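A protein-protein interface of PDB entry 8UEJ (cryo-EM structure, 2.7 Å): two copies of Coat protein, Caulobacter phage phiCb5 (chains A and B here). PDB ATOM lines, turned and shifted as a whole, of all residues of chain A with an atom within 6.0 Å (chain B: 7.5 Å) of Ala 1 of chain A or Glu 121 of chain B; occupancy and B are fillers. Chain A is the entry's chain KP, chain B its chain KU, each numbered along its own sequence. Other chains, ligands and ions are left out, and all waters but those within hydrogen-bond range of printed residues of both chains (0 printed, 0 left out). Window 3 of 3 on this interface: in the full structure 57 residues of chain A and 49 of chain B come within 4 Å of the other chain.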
ATOM      1  N   ALA A   1      19.790 -13.681  21.395  1.00  0.00           N
ATOM      2  CA  ALA A   1      19.360 -12.603  20.459  1.00  0.00           C
ATOM      3  C   ALA A   1      20.343 -11.440  20.494  1.00  0.00           C
ATOM      4  O   ALA A   1      19.947 -10.279  20.440  1.00  0.00           O
ATOM      5  CB  ALA A   1      17.961 -12.128  20.809  1.00  0.00           C
ATOM      6  N   LEU A   2      21.634 -11.767  20.582  1.00  0.00           N
ATOM      7  CA  LEU A   2      22.658 -10.730  20.627  1.00  0.00           C
ATOM      8  C   LEU A   2      22.688  -9.932  19.328  1.00  0.00           C
ATOM      9  O   LEU A   2      22.834  -8.705  19.348  1.00  0.00           O
ATOM     10  CB  LEU A   2      24.026 -11.360  20.897  1.00  0.00           C
ATOM     11  CG  LEU A   2      24.388 -11.671  22.353  1.00  0.00           C
ATOM     12  CD1 LEU A   2      24.474 -10.397  23.172  1.00  0.00           C
ATOM     13  CD2 LEU A   2      23.384 -12.642  22.964  1.00  0.00           C
ATOM     14  N   GLY A   3      22.539 -10.608  18.192  1.00  0.00           N
ATOM     15  CA  GLY A   3      22.602  -9.952  16.901  1.00  0.00           C
ATOM     16  C   GLY A   3      23.363 -10.772  15.882  1.00  0.00           C
ATOM     17  O   GLY A   3      24.105 -11.691  16.243  1.00  0.00           O
ATOM     18  N   LYS A  22      27.305 -14.409  12.425  1.00  0.00           N
ATOM     19  CA  LYS A  22      26.712 -15.617  12.981  1.00  0.00           C
ATOM     20  C   LYS A  22      26.828 -16.785  12.009  1.00  0.00           C
ATOM     21  O   LYS A  22      26.672 -16.629  10.796  1.00  0.00           O
ATOM     22  CB  LYS A  22      25.248 -15.380  13.363  1.00  0.00           C
ATOM     23  CG  LYS A  22      24.628 -16.584  14.068  1.00  0.00           C
ATOM     24  CD  LYS A  22      23.157 -16.405  14.415  1.00  0.00           C
ATOM     25  CE  LYS A  22      22.990 -15.450  15.583  1.00  0.00           C
ATOM     26  NZ  LYS A  22      21.576 -15.340  16.037  1.00  0.00           N
ATOM     27  N   GLN A  25      23.507 -21.916  15.571  1.00  0.00           N
ATOM     28  CA  GLN A  25      22.723 -21.747  16.790  1.00  0.00           C
ATOM     29  C   GLN A  25      22.061 -23.079  17.102  1.00  0.00           C
ATOM     30  O   GLN A  25      21.097 -23.459  16.434  1.00  0.00           O
ATOM     31  CB  GLN A  25      21.689 -20.645  16.635  1.00  0.00           C
ATOM     32  CG  GLN A  25      20.921 -20.386  17.915  1.00  0.00           C
ATOM     33  CD  GLN A  25      19.933 -19.256  17.789  1.00  0.00           C
ATOM     34  OE1 GLN A  25      19.778 -18.666  16.721  1.00  0.00           O
ATOM     35  NE2 GLN A  25      19.262 -18.940  18.886  1.00  0.00           N
ATOM     36  N   TYR A  28      20.797 -23.649  22.612  1.00  0.00           N
ATOM     37  CA  TYR A  28      21.018 -22.427  23.384  1.00  0.00           C
ATOM     38  C   TYR A  28      22.460 -21.934  23.271  1.00  0.00           C
ATOM     39  O   TYR A  28      22.974 -21.278  24.181  1.00  0.00           O
ATOM     40  CB  TYR A  28      20.650 -22.632  24.856  1.00  0.00           C
ATOM     41  CG  TYR A  28      19.249 -23.145  25.064  1.00  0.00           C
ATOM     42  CD1 TYR A  28      18.980 -24.503  25.039  1.00  0.00           C
ATOM     43  CD2 TYR A  28      18.192 -22.275  25.275  1.00  0.00           C
ATOM     44  CE1 TYR A  28      17.703 -24.976  25.224  1.00  0.00           C
ATOM     45  CE2 TYR A  28      16.914 -22.743  25.460  1.00  0.00           C
ATOM     46  CZ  TYR A  28      16.673 -24.093  25.433  1.00  0.00           C
ATOM     47  OH  TYR A  28      15.393 -24.571  25.617  1.00  0.00           O
ATOM     48  N   VAL A  45      28.987 -18.683  22.599  1.00  0.00           N
ATOM     49  CA  VAL A  45      28.218 -18.351  23.790  1.00  0.00           C
ATOM     50  C   VAL A  45      27.364 -19.562  24.130  1.00  0.00           C
ATOM     51  O   VAL A  45      26.704 -20.120  23.248  1.00  0.00           O
ATOM     52  CB  VAL A  45      27.344 -17.103  23.577  1.00  0.00           C
ATOM     53  CG1 VAL A  45      26.559 -16.790  24.839  1.00  0.00           C
ATOM     54  CG2 VAL A  45      28.217 -15.926  23.149  1.00  0.00           C
ATOM     55  N   HIS A  47      24.929 -21.723  27.400  1.00  0.00           N
ATOM     56  CA  HIS A  47      24.211 -21.771  28.666  1.00  0.00           C
ATOM     57  C   HIS A  47      23.963 -23.229  29.029  1.00  0.00           C
ATOM     58  O   HIS A  47      23.795 -24.076  28.149  1.00  0.00           O
ATOM     59  CB  HIS A  47      22.868 -21.039  28.585  1.00  0.00           C
ATOM     60  CG  HIS A  47      22.954 -19.665  27.998  1.00  0.00           C
ATOM     61  ND1 HIS A  47      23.492 -18.595  28.679  1.00  0.00           N
ATOM     62  CD2 HIS A  47      22.572 -19.189  26.791  1.00  0.00           C
ATOM     63  CE1 HIS A  47      23.431 -17.517  27.918  1.00  0.00           C
ATOM     64  NE2 HIS A  47      22.877 -17.850  26.767  1.00  0.00           N
ATOM     65  N   LEU B 113      25.658  -6.401  28.763  1.00  0.00           N
ATOM     66  CA  LEU B 113      25.855  -7.765  28.294  1.00  0.00           C
ATOM     67  C   LEU B 113      25.631  -8.773  29.407  1.00  0.00           C
ATOM     68  O   LEU B 113      25.108  -9.861  29.151  1.00  0.00           O
ATOM     69  CB  LEU B 113      27.255  -7.936  27.703  1.00  0.00           C
ATOM     70  CG  LEU B 113      27.477  -9.289  27.022  1.00  0.00           C
ATOM     71  CD1 LEU B 113      28.516  -9.178  25.951  1.00  0.00           C
ATOM     72  CD2 LEU B 113      27.915 -10.355  28.031  1.00  0.00           C
ATOM     73  N   GLY B 115      23.521  -8.471  31.834  1.00  0.00           N
ATOM     74  CA  GLY B 115      22.075  -8.600  31.889  1.00  0.00           C
ATOM     75  C   GLY B 115      21.528  -9.497  30.795  1.00  0.00           C
ATOM     76  O   GLY B 115      20.694 -10.369  31.051  1.00  0.00           O
ATOM     77  N   LYS B 116      22.001  -9.307  29.560  1.00  0.00           N
ATOM     78  CA  LYS B 116      21.568 -10.188  28.476  1.00  0.00           C
ATOM     79  C   LYS B 116      21.914 -11.642  28.774  1.00  0.00           C
ATOM     80  O   LYS B 116      21.095 -12.540  28.546  1.00  0.00           O
ATOM     81  CB  LYS B 116      22.190  -9.769  27.140  1.00  0.00           C
ATOM     82  CG  LYS B 116      22.157  -8.283  26.812  1.00  0.00           C
ATOM     83  CD  LYS B 116      20.883  -7.899  26.084  1.00  0.00           C
ATOM     84  CE  LYS B 116      21.063  -6.619  25.281  1.00  0.00           C
ATOM     85  NZ  LYS B 116      22.096  -6.765  24.214  1.00  0.00           N
ATOM     86  N   LEU B 117      23.125 -11.895  29.274  1.00  0.00           N
ATOM     87  CA  LEU B 117      23.543 -13.267  29.543  1.00  0.00           C
ATOM     88  C   LEU B 117      22.659 -13.910  30.600  1.00  0.00           C
ATOM     89  O   LEU B 117      22.228 -15.059  30.447  1.00  0.00           O
ATOM     90  CB  LEU B 117      25.001 -13.289  29.994  1.00  0.00           C
ATOM     91  CG  LEU B 117      26.122 -13.374  28.950  1.00  0.00           C
ATOM     92  CD1 LEU B 117      27.428 -13.714  29.652  1.00  0.00           C
ATOM     93  CD2 LEU B 117      25.846 -14.389  27.849  1.00  0.00           C
ATOM     94  N   ILE B 118      22.363 -13.179  31.677  1.00  0.00           N
ATOM     95  CA  ILE B 118      21.407 -13.687  32.655  1.00  0.00           C
ATOM     96  C   ILE B 118      20.054 -13.900  31.999  1.00  0.00           C
ATOM     97  O   ILE B 118      19.273 -14.756  32.428  1.00  0.00           O
ATOM     98  CB  ILE B 118      21.308 -12.738  33.864  1.00  0.00           C
ATOM     99  CG1 ILE B 118      22.673 -12.583  34.546  1.00  0.00           C
ATOM    100  CG2 ILE B 118      20.261 -13.240  34.847  1.00  0.00           C
ATOM    101  CD1 ILE B 118      23.295 -13.887  35.022  1.00  0.00           C
ATOM    102  N   GLY B 119      19.754 -13.139  30.952  1.00  0.00           N
ATOM    103  CA  GLY B 119      18.511 -13.332  30.228  1.00  0.00           C
ATOM    104  C   GLY B 119      18.458 -14.562  29.349  1.00  0.00           C
ATOM    105  O   GLY B 119      17.448 -14.765  28.670  1.00  0.00           O
ATOM    106  N   TRP B 120      19.512 -15.380  29.321  1.00  0.00           N
ATOM    107  CA  TRP B 120      19.599 -16.586  28.499  1.00  0.00           C
ATOM    108  C   TRP B 120      19.677 -16.266  27.013  1.00  0.00           C
ATOM    109  O   TRP B 120      19.477 -17.155  26.179  1.00  0.00           O
ATOM    110  CB  TRP B 120      18.437 -17.547  28.786  1.00  0.00           C
ATOM    111  CG  TRP B 120      18.732 -18.451  29.938  1.00  0.00           C
ATOM    112  CD1 TRP B 120      18.695 -18.129  31.264  1.00  0.00           C
ATOM    113  CD2 TRP B 120      19.078 -19.840  29.873  1.00  0.00           C
ATOM    114  NE1 TRP B 120      19.026 -19.225  32.026  1.00  0.00           N
ATOM    115  CE2 TRP B 120      19.258 -20.288  31.196  1.00  0.00           C
ATOM    116  CE3 TRP B 120      19.258 -20.748  28.823  1.00  0.00           C
ATOM    117  CZ2 TRP B 120      19.612 -21.601  31.497  1.00  0.00           C
ATOM    118  CZ3 TRP B 120      19.610 -22.048  29.126  1.00  0.00           C
ATOM    119  CH2 TRP B 120      19.783 -22.463  30.453  1.00  0.00           C
ATOM    120  N   GLU B 121      19.954 -15.013  26.661  1.00  0.00           N
ATOM    121  CA  GLU B 121      20.271 -14.676  25.282  1.00  0.00           C
ATOM    122  C   GLU B 121      21.510 -15.441  24.839  1.00  0.00           C
ATOM    123  O   GLU B 121      22.485 -15.559  25.586  1.00  0.00           O
ATOM    124  CB  GLU B 121      20.511 -13.176  25.153  1.00  0.00           C
ATOM    125  CG  GLU B 121      19.265 -12.363  24.873  1.00  0.00           C
ATOM    126  CD  GLU B 121      18.529 -11.995  26.141  1.00  0.00           C
ATOM    127  OE1 GLU B 121      18.596 -12.775  27.114  1.00  0.00           O
ATOM    128  OE2 GLU B 121      17.891 -10.922  26.173  1.00  0.00           O
ATOM    129  N   SER B 122      21.468 -15.961  23.617  1.00  0.00           N
ATOM    130  CA  SER B 122      22.573 -16.753  23.092  1.00  0.00           C
ATOM    131  C   SER B 122      23.129 -16.125  21.823  1.00  0.00           C
ATOM    132  O   SER B 122      24.256 -16.402  21.425  1.00  0.00           O
ATOM    133  CB  SER B 122      22.113 -18.186  22.821  1.00  0.00           C
ATOM    134  OG  SER B 122      23.162 -18.965  22.273  1.00  0.00           O
ATOM    135  OXT SER B 122      22.463 -15.323  21.167  1.00  0.00           O
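Of the printed residues of chain B, Ala 1 of chain A touches Glu 121 and Ser 122. Glu 121 of chain B touches three residues of chain A. Of the printed residues of chain B, Leu 2 of chain A touches Glu 121 (3.7 Å) and Ser 122 (3.4 Å). Printed residues of chain B within 4 Å of Tyr 28 of chain A: Ser 122. Printed residues of chain A within 4 Å of Ser 122 of chain B: Ala 1 (3.1 Å), Leu 2 (3.4 Å), Tyr 28 (3.0 Å), Val 45 (3.8 Å) and His 47 (3.8 Å). Printed residues of chain B within 4 Å of Val 45 of chain A: Leu 117 and Ser 122. Of the printed residues of chain B, His 47 of chain A touches Leu 117 (3.7 Å), Trp 120 (3.5 Å), Glu 121 (2.6 Å) and Ser 122 (3.8 Å). Leu 113 of chain B touches none of the printed residues of chain A. The nearest residue of chain B that does not touch Ala 1 of chain A is Lys 116 of chain B (5.6 Å).
Printed residues of chain B that touch a printed residue of chain A: Leu 117, Trp 120, Glu 121 and Ser 122. Hydrophobic or aromatic side chains of chain B within 4 Å of the printed part of chain A: Leu 117 and Trp 120. Of the 8 printed residues of chain A, 5 touch a printed residue of chain B. Hydrophobic or aromatic side chains of chain A that line the printed part of chain B: Leu 2, Val 45 and His 47.
N of Ala 1 of chain A touches CG of Glu 121 of chain B, at 3.8 Å. Leu 2 of chain A touches Glu 121 of chain B (CD2 to CB, 3.7 Å). OXT of Ser 122 of chain B touches CD2 of Leu 2 of chain A, 3.4 Å away. Val 45 of chain A touches Leu 117 of chain B. CB of Val 45 of chain A touches O of Ser 122 of chain B (3.8 Å). His 47 of chain A touches Leu 117 of chain B. His 47 of chain A touches Trp 120 of chain B. NE2 of His 47 of chain A touches CA of Ser 122 of chain B (3.8 Å).
The backbone NH (N) of Ala 1 of chain A lies within hydrogen-bond range of the chain-end carboxylate (OXT) of Ser 122 of chain B (3.1 Å). The backbone carbonyl oxygen (O) of Tyr 28 of chain A lies within hydrogen-bond range of the side-chain hydroxyl (OG) of Ser 122 of chain B. A ring nitrogen (NE2) of His 47 of chain A is in hydrogen-bond range of the backbone carbonyl oxygen (O) of Glu 121 of chain B, at 2.6 Å.
No position is printed for both chains.
The backbone NH (N) of Glu 121 of chain B is in hydrogen-bond range of the backbone carbonyl oxygen (O) of Lys 116 of chain B (3.3 Å).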
